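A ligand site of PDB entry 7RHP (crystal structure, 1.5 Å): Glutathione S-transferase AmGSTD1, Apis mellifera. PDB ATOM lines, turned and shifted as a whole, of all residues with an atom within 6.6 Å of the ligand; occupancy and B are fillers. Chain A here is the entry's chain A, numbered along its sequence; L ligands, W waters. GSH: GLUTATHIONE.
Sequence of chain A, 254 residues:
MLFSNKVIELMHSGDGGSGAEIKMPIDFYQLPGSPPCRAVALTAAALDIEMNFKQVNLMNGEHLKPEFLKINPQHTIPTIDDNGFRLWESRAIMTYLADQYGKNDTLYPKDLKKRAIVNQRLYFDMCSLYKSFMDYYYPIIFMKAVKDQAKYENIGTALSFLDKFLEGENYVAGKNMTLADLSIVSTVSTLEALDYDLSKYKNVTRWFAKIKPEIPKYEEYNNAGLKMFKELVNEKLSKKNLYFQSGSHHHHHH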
ATOM      1  N   LEU A  31     -13.722 -15.333  19.110  1.00  0.00           N
ATOM      2  CA  LEU A  31     -15.071 -14.782  19.082  1.00  0.00           C
ATOM      3  C   LEU A  31     -15.575 -15.065  17.671  1.00  0.00           C
ATOM      4  O   LEU A  31     -14.913 -14.693  16.696  1.00  0.00           O
ATOM      5  CB  LEU A  31     -15.103 -13.279  19.373  1.00  0.00           C
ATOM      6  CG  LEU A  31     -16.481 -12.670  19.578  1.00  0.00           C
ATOM      7  CD1 LEU A  31     -17.146 -13.205  20.820  1.00  0.00           C
ATOM      8  CD2 LEU A  31     -16.332 -11.149  19.652  1.00  0.00           C
ATOM      9  N   SER A  34     -15.235 -12.665  14.526  1.00  0.00           N
ATOM     10  CA  SER A  34     -13.996 -11.926  14.310  1.00  0.00           C
ATOM     11  C   SER A  34     -13.241 -12.422  13.081  1.00  0.00           C
ATOM     12  O   SER A  34     -12.934 -13.624  13.010  1.00  0.00           O
ATOM     13  CB  SER A  34     -13.119 -12.051  15.544  1.00  0.00           C
ATOM     14  OG  SER A  34     -11.774 -11.717  15.256  1.00  0.00           O
ATOM     15  N   PRO A  35     -12.915 -11.560  12.119  1.00  0.00           N
ATOM     16  CA  PRO A  35     -12.232 -12.038  10.904  1.00  0.00           C
ATOM     17  C   PRO A  35     -10.938 -12.774  11.207  1.00  0.00           C
ATOM     18  O   PRO A  35     -10.710 -13.858  10.633  1.00  0.00           O
ATOM     19  CB  PRO A  35     -11.982 -10.748  10.105  1.00  0.00           C
ATOM     20  CG  PRO A  35     -13.098  -9.802  10.556  1.00  0.00           C
ATOM     21  CD  PRO A  35     -13.302 -10.142  12.024  1.00  0.00           C
ATOM     22  N   PRO A  36     -10.053 -12.244  12.052  1.00  0.00           N
ATOM     23  CA  PRO A  36      -8.802 -12.989  12.296  1.00  0.00           C
ATOM     24  C   PRO A  36      -9.040 -14.321  12.996  1.00  0.00           C
ATOM     25  O   PRO A  36      -8.314 -15.297  12.730  1.00  0.00           O
ATOM     26  CB  PRO A  36      -7.963 -12.013  13.157  1.00  0.00           C
ATOM     27  CG  PRO A  36      -8.982 -11.133  13.836  1.00  0.00           C
ATOM     28  CD  PRO A  36     -10.047 -10.941  12.742  1.00  0.00           C
ATOM     29  N   CYS A  37     -10.042 -14.406  13.874  1.00  0.00           N
ATOM     30  CA  CYS A  37     -10.379 -15.728  14.417  1.00  0.00           C
ATOM     31  C   CYS A  37     -10.885 -16.686  13.340  1.00  0.00           C
ATOM     32  O   CYS A  37     -10.517 -17.863  13.345  1.00  0.00           O
ATOM     33  CB  CYS A  37     -11.392 -15.661  15.569  1.00  0.00           C
ATOM     34  SG  CYS A  37     -10.887 -14.722  17.013  1.00  0.00           S
ATOM     35  N   LEU A  58     -15.476 -10.204  24.077  1.00  0.00           N
ATOM     36  CA  LEU A  58     -14.837  -8.898  24.129  1.00  0.00           C
ATOM     37  C   LEU A  58     -15.812  -7.807  24.555  1.00  0.00           C
ATOM     38  O   LEU A  58     -15.387  -6.792  25.128  1.00  0.00           O
ATOM     39  CB  LEU A  58     -14.252  -8.551  22.757  1.00  0.00           C
ATOM     40  CG  LEU A  58     -13.256  -9.525  22.140  1.00  0.00           C
ATOM     41  CD1 LEU A  58     -12.797  -9.014  20.772  1.00  0.00           C
ATOM     42  CD2 LEU A  58     -12.074  -9.732  23.042  1.00  0.00           C
ATOM     43  N   HIS A  63     -11.513 -10.466  27.897  1.00  0.00           N
ATOM     44  CA  HIS A  63     -10.100 -10.464  27.535  1.00  0.00           C
ATOM     45  C   HIS A  63      -9.253  -9.603  28.458  1.00  0.00           C
ATOM     46  O   HIS A  63      -8.024  -9.665  28.386  1.00  0.00           O
ATOM     47  CB  HIS A  63      -9.926  -9.998  26.097  1.00  0.00           C
ATOM     48  CG  HIS A  63     -10.464  -8.628  25.837  1.00  0.00           C
ATOM     49  ND1 HIS A  63     -11.767  -8.263  26.089  1.00  0.00           N
ATOM     50  CD2 HIS A  63      -9.869  -7.512  25.343  1.00  0.00           C
ATOM     51  CE1 HIS A  63     -11.964  -7.003  25.745  1.00  0.00           C
ATOM     52  NE2 HIS A  63     -10.822  -6.521  25.281  1.00  0.00           N
ATOM     53  N   LEU A  64      -9.876  -8.813  29.320  1.00  0.00           N
ATOM     54  CA  LEU A  64      -9.149  -7.947  30.226  1.00  0.00           C
ATOM     55  C   LEU A  64      -9.133  -8.486  31.658  1.00  0.00           C
ATOM     56  O   LEU A  64      -8.593  -7.829  32.549  1.00  0.00           O
ATOM     57  CB  LEU A  64      -9.779  -6.551  30.205  1.00  0.00           C
ATOM     58  CG  LEU A  64      -9.979  -5.945  28.811  1.00  0.00           C
ATOM     59  CD1 LEU A  64     -10.868  -4.712  28.866  1.00  0.00           C
ATOM     60  CD2 LEU A  64      -8.630  -5.619  28.193  1.00  0.00           C
ATOM     61  N   GLN A  74      -1.178  -8.889  25.808  1.00  0.00           N
ATOM     62  CA  GLN A  74      -1.693  -7.949  24.812  1.00  0.00           C
ATOM     63  C   GLN A  74      -3.207  -7.994  24.720  1.00  0.00           C
ATOM     64  O   GLN A  74      -3.788  -7.133  24.039  1.00  0.00           O
ATOM     65  CB  GLN A  74      -1.055  -8.257  23.458  1.00  0.00           C
ATOM     66  CG  GLN A  74      -1.088  -7.120  22.466  1.00  0.00           C
ATOM     67  CD  GLN A  74      -0.378  -7.460  21.167  1.00  0.00           C
ATOM     68  OE1 GLN A  74       0.547  -8.286  21.113  1.00  0.00           O
ATOM     69  NE2 GLN A  74      -0.793  -6.803  20.102  1.00  0.00           N
ATOM     70  N   HIS A  75      -3.843  -8.934  25.416  1.00  0.00           N
ATOM     71  CA  HIS A  75      -5.292  -9.120  25.470  1.00  0.00           C
ATOM     72  C   HIS A  75      -5.947  -8.991  24.095  1.00  0.00           C
ATOM     73  O   HIS A  75      -6.900  -8.227  23.887  1.00  0.00           O
ATOM     74  CB  HIS A  75      -5.953  -8.181  26.509  1.00  0.00           C
ATOM     75  CG  HIS A  75      -5.552  -6.733  26.420  1.00  0.00           C
ATOM     76  ND1 HIS A  75      -6.146  -5.845  25.547  1.00  0.00           N
ATOM     77  CD2 HIS A  75      -4.663  -6.015  27.137  1.00  0.00           C
ATOM     78  CE1 HIS A  75      -5.617  -4.650  25.706  1.00  0.00           C
ATOM     79  NE2 HIS A  75      -4.710  -4.723  26.666  1.00  0.00           N
ATOM     80  N   THR A  76      -5.480  -9.818  23.172  1.00  0.00           N
ATOM     81  CA  THR A  76      -6.070  -9.913  21.846  1.00  0.00           C
ATOM     82  C   THR A  76      -6.529 -11.337  21.551  1.00  0.00           C
ATOM     83  O   THR A  76      -5.982 -12.321  22.080  1.00  0.00           O
ATOM     84  CB  THR A  76      -5.112  -9.457  20.734  1.00  0.00           C
ATOM     85  OG1 THR A  76      -3.896 -10.215  20.786  1.00  0.00           O
ATOM     86  CG2 THR A  76      -4.779  -7.968  20.859  1.00  0.00           C
ATOM     87  N   ILE A  77      -7.537 -11.437  20.698  1.00  0.00           N
ATOM     88  CA  ILE A  77      -7.908 -12.711  20.095  1.00  0.00           C
ATOM     89  C   ILE A  77      -7.716 -12.577  18.585  1.00  0.00           C
ATOM     90  O   ILE A  77      -7.861 -11.472  18.034  1.00  0.00           O
ATOM     91  CB  ILE A  77      -9.337 -13.140  20.455  1.00  0.00           C
ATOM     92  CG1 ILE A  77     -10.349 -12.054  20.115  1.00  0.00           C
ATOM     93  CG2 ILE A  77      -9.404 -13.546  21.941  1.00  0.00           C
ATOM     94  CD1 ILE A  77     -11.787 -12.501  20.306  1.00  0.00           C
ATOM     95  N   PRO A  78      -7.408 -13.656  17.870  1.00  0.00           N
ATOM     96  CA  PRO A  78      -7.260 -15.013  18.404  1.00  0.00           C
ATOM     97  C   PRO A  78      -5.959 -15.226  19.168  1.00  0.00           C
ATOM     98  O   PRO A  78      -4.934 -14.610  18.867  1.00  0.00           O
ATOM     99  CB  PRO A  78      -7.284 -15.891  17.145  1.00  0.00           C
ATOM    100  CG  PRO A  78      -6.701 -14.994  16.093  1.00  0.00           C
ATOM    101  CD  PRO A  78      -7.247 -13.622  16.409  1.00  0.00           C
ATOM    102  N   TRP A  88      -0.170 -15.634  19.708  1.00  0.00           N
ATOM    103  CA  TRP A  88      -1.198 -14.795  19.112  1.00  0.00           C
ATOM    104  C   TRP A  88      -0.635 -14.150  17.836  1.00  0.00           C
ATOM    105  O   TRP A  88       0.480 -14.491  17.417  1.00  0.00           O
ATOM    106  CB  TRP A  88      -1.732 -13.772  20.134  1.00  0.00           C
ATOM    107  CG  TRP A  88      -0.742 -12.951  20.885  1.00  0.00           C
ATOM    108  CD1 TRP A  88      -0.385 -11.663  20.626  1.00  0.00           C
ATOM    109  CD2 TRP A  88      -0.019 -13.347  22.055  1.00  0.00           C
ATOM    110  NE1 TRP A  88       0.536 -11.240  21.548  1.00  0.00           N
ATOM    111  CE2 TRP A  88       0.779 -12.249  22.440  1.00  0.00           C
ATOM    112  CE3 TRP A  88       0.044 -14.522  22.817  1.00  0.00           C
ATOM    113  CZ2 TRP A  88       1.626 -12.289  23.551  1.00  0.00           C
ATOM    114  CZ3 TRP A  88       0.894 -14.558  23.909  1.00  0.00           C
ATOM    115  CH2 TRP A  88       1.676 -13.464  24.260  1.00  0.00           C
ATOM    116  N   GLU A  89      -1.396 -13.241  17.230  1.00  0.00           N
ATOM    117  CA  GLU A  89      -1.249 -12.831  15.828  1.00  0.00           C
ATOM    118  C   GLU A  89      -1.762 -13.942  14.907  1.00  0.00           C
ATOM    119  O   GLU A  89      -1.087 -14.961  14.707  1.00  0.00           O
ATOM    120  CB  GLU A  89       0.196 -12.476  15.477  1.00  0.00           C
ATOM    121  CG  GLU A  89       0.685 -11.178  16.112  1.00  0.00           C
ATOM    122  CD  GLU A  89      -0.082  -9.938  15.641  1.00  0.00           C
ATOM    123  OE1 GLU A  89      -0.770  -9.975  14.600  1.00  0.00           O
ATOM    124  OE2 GLU A  89       0.044  -8.903  16.339  1.00  0.00           O
ATOM    125  N   SER A  90      -2.951 -13.730  14.354  1.00  0.00           N
ATOM    126  CA  SER A  90      -3.646 -14.769  13.605  1.00  0.00           C
ATOM    127  C   SER A  90      -2.758 -15.411  12.542  1.00  0.00           C
ATOM    128  O   SER A  90      -2.736 -16.638  12.404  1.00  0.00           O
ATOM    129  CB  SER A  90      -4.898 -14.180  12.950  1.00  0.00           C
ATOM    130  OG  SER A  90      -4.594 -13.035  12.163  1.00  0.00           O
ATOM    131  N   ARG A  91      -2.053 -14.606  11.747  1.00  0.00           N
ATOM    132  CA  ARG A  91      -1.297 -15.176  10.638  1.00  0.00           C
ATOM    133  C   ARG A  91      -0.058 -15.934  11.114  1.00  0.00           C
ATOM    134  O   ARG A  91       0.371 -16.870  10.443  1.00  0.00           O
ATOM    135  CB  ARG A  91      -0.967 -14.063   9.642  1.00  0.00           C
ATOM    136  CG  ARG A  91      -2.115 -13.771   8.669  1.00  0.00           C
ATOM    137  CD  ARG A  91      -3.471 -13.556   9.337  1.00  0.00           C
ATOM    138  NE  ARG A  91      -4.505 -13.241   8.343  1.00  0.00           N
ATOM    139  CZ  ARG A  91      -5.753 -12.865   8.636  1.00  0.00           C
ATOM    140  NH1 ARG A  91      -6.141 -12.724   9.892  1.00  0.00           N
ATOM    141  NH2 ARG A  91      -6.620 -12.587   7.670  1.00  0.00           N
ATOM    142  N   ILE A  93      -0.218 -17.704  13.931  1.00  0.00           N
ATOM    143  CA  ILE A  93      -0.876 -18.954  14.330  1.00  0.00           C
ATOM    144  C   ILE A  93      -1.089 -19.850  13.121  1.00  0.00           C
ATOM    145  O   ILE A  93      -0.840 -21.064  13.173  1.00  0.00           O
ATOM    146  CB  ILE A  93      -2.203 -18.656  15.038  1.00  0.00           C
ATOM    147  CG1 ILE A  93      -1.977 -17.959  16.385  1.00  0.00           C
ATOM    148  CG2 ILE A  93      -2.996 -19.964  15.221  1.00  0.00           C
ATOM    149  CD1 ILE A  93      -3.284 -17.398  16.941  1.00  0.00           C
ATOM    150  N   MET A 126      -2.913  -8.363   5.900  1.00  0.00           N
ATOM    151  CA  MET A 126      -2.943  -7.695   7.195  1.00  0.00           C
ATOM    152  C   MET A 126      -2.629  -6.212   7.090  1.00  0.00           C
ATOM    153  O   MET A 126      -3.189  -5.426   7.857  1.00  0.00           O
ATOM    154  CB  MET A 126      -1.980  -8.370   8.161  1.00  0.00           C
ATOM    155  CG  MET A 126      -2.387  -9.805   8.447  1.00  0.00           C
ATOM    156  SD  MET A 126      -3.960  -9.957   9.343  1.00  0.00           S
ATOM    157  CE  MET A 126      -5.199  -9.962   8.064  1.00  0.00           C
ATOM    158  N   TYR A 130      -7.230  -6.205   5.062  1.00  0.00           N
ATOM    159  CA  TYR A 130      -7.921  -6.179   6.355  1.00  0.00           C
ATOM    160  C   TYR A 130      -7.749  -4.824   7.028  1.00  0.00           C
ATOM    161  O   TYR A 130      -8.705  -4.280   7.600  1.00  0.00           O
ATOM    162  CB  TYR A 130      -7.399  -7.323   7.241  1.00  0.00           C
ATOM    163  CG  TYR A 130      -8.044  -7.395   8.615  1.00  0.00           C
ATOM    164  CD1 TYR A 130      -9.413  -7.538   8.761  1.00  0.00           C
ATOM    165  CD2 TYR A 130      -7.278  -7.298   9.761  1.00  0.00           C
ATOM    166  CE1 TYR A 130     -10.010  -7.587  10.012  1.00  0.00           C
ATOM    167  CE2 TYR A 130      -7.864  -7.365  11.000  1.00  0.00           C
ATOM    168  CZ  TYR A 130      -9.221  -7.498  11.140  1.00  0.00           C
ATOM    169  OH  TYR A 130      -9.740  -7.551  12.412  1.00  0.00           O
ATOM    170  N   MET A 134     -10.897  -2.556   8.311  1.00  0.00           N
ATOM    171  CA  MET A 134     -11.092  -2.159   9.704  1.00  0.00           C
ATOM    172  C   MET A 134     -11.046  -0.643   9.865  1.00  0.00           C
ATOM    173  O   MET A 134     -11.861  -0.070  10.597  1.00  0.00           O
ATOM    174  CB  MET A 134     -10.047  -2.811  10.595  1.00  0.00           C
ATOM    175  CG  MET A 134     -10.359  -4.249  10.996  1.00  0.00           C
ATOM    176  SD  MET A 134     -11.947  -4.442  11.842  1.00  0.00           S
ATOM    177  CE  MET A 134     -11.509  -3.952  13.509  1.00  0.00           C
HETATM  178  N1  GSH L   1      -3.080  -8.387  14.219  1.00  0.00           N
HETATM  179  CA1 GSH L   1      -3.912  -9.153  15.136  1.00  0.00           C
HETATM  180  C1  GSH L   1      -4.209 -10.525  14.555  1.00  0.00           C
HETATM  181  O11 GSH L   1      -4.185 -10.673  13.307  1.00  0.00           O
HETATM  182  O12 GSH L   1      -4.450 -11.492  15.314  1.00  0.00           O
HETATM  183  CB1 GSH L   1      -5.205  -8.394  15.351  1.00  0.00           C
HETATM  184  CG1 GSH L   1      -5.971  -9.060  16.482  1.00  0.00           C
HETATM  185  CD1 GSH L   1      -7.097  -8.153  16.923  1.00  0.00           C
HETATM  186  OE1 GSH L   1      -7.177  -7.016  16.573  1.00  0.00           O
HETATM  187  N2  GSH L   1      -8.077  -8.745  17.791  1.00  0.00           N
HETATM  188  CA2 GSH L   1      -9.183  -7.978  18.270  1.00  0.00           C
HETATM  189  C2  GSH L   1      -9.075  -7.904  19.791  1.00  0.00           C
HETATM  190  O2  GSH L   1      -8.797  -8.876  20.438  1.00  0.00           O
HETATM  191  CB2 GSH L   1     -10.491  -8.696  17.956  1.00  0.00           C
HETATM  192  SG2 GSH L   1     -10.825  -8.718  16.177  1.00  0.00           S
HETATM  193  N3  GSH L   1      -9.338  -6.631  20.447  1.00  0.00           N
HETATM  194  CA3 GSH L   1      -9.269  -6.533  21.894  1.00  0.00           C
HETATM  195  C3  GSH L   1      -8.032  -5.783  22.368  1.00  0.00           C
HETATM  196  O31 GSH L   1      -7.088  -5.523  21.587  1.00  0.00           O
HETATM  197  O32 GSH L   1      -7.952  -5.436  23.577  1.00  0.00           O
HETATM  198  O   HOH W   1      -2.984  -5.732  15.662  1.00  0.00           O
HETATM  199  O   HOH W   2      -4.346  -6.093  12.745  1.00  0.00           O
HETATM  200  O   HOH W   3      -4.506  -4.983  22.585  1.00  0.00           O
HETATM  201  O   HOH W   4     -10.082  -4.339  18.626  1.00  0.00           O
HETATM  202  O   HOH W   5      -4.097 -12.123  17.948  1.00  0.00           O
HETATM  203  O   HOH W   6      -9.128  -2.860  23.814  1.00  0.00           O
HETATM  204  O   HOH W   7      -7.498  -5.642  14.207  1.00  0.00           O
HETATM  205  O   HOH W   8      -1.501 -11.614  12.096  1.00  0.00           O
HETATM  206  O   HOH W   9      -6.751  -4.816  18.881  1.00  0.00           O
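An oxygen (O12) of the ligand sits at hydrogen-bond distance from the backbone NH (N) of Ser 90, 2.9 Å away. The side-chain hydroxyl of Ser 90 lies within hydrogen-bond range of an oxygen (O11) of the ligand (2.7 Å). O of His 75 sits close to O32 of the ligand (3.0 Å). A ring nitrogen (ND1) of His 75 lies within hydrogen-bond range of an oxygen (O32) of the ligand. The backbone NH of Ile 77 sits at hydrogen-bond distance from an oxygen (O2) of the ligand (2.9 Å). N2 of the ligand is in hydrogen-bond range of O of Ile 77 (2.7 Å). A nitrogen (N1) of the ligand is in salt-bridge range of the side-chain carboxylate (OE1) of Glu 89, 2.8 Å away. OG of Ser 34 sits close to SG2 of the ligand (3.3 Å).
NH1 of Arg 91 is in hydrogen-bond range of OG of Ser 90, 2.8 Å away. The side-chain hydroxyl (OG) of Ser 34 sits at hydrogen-bond distance from the backbone NH (N) of Cys 37 (3.5 Å).
Pro 36 touches the ligand (CG to SG2, 3.8 Å). Leu 58 touches the ligand. CD2 of His 63 touches O32 of the ligand, 3.3 Å away. Thr 76 touches the ligand (CA to O2, 3.2 Å). Pro 78 touches the ligand (CD to O12, 3.7 Å). Hydrophobic or aromatic side chains that line the ligand: Pro 36, Leu 58, His 63, His 75, Ile 77 and Pro 78.
Water W5 lies within hydrogen-bond range of an oxygen (O12) of the ligand (2.7 Å), the backbone carbonyl oxygen (O) of Pro 78 (2.8 Å), the backbone NH (N) of Glu 89 (3.0 Å) and the side-chain hydroxyl (OG1) of Thr 76 (3.4 Å). Water W7 bridges OE1 of the ligand and OH of Tyr 130. Water W3 lies within hydrogen-bond range of O of Gln 74 (2.7 Å), O31 of the ligand (2.8 Å) and ND1 of His 75 (3.5 Å). Water W8 lies within hydrogen-bond range of the backbone NH (N) of Arg 91 (3.1 Å), the side-chain carboxylate (OE1) of Glu 89 (3.1 Å), an oxygen (O11) of the ligand (3.1 Å) and the side-chain hydroxyl (OG) of Ser 90 (3.4 Å).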
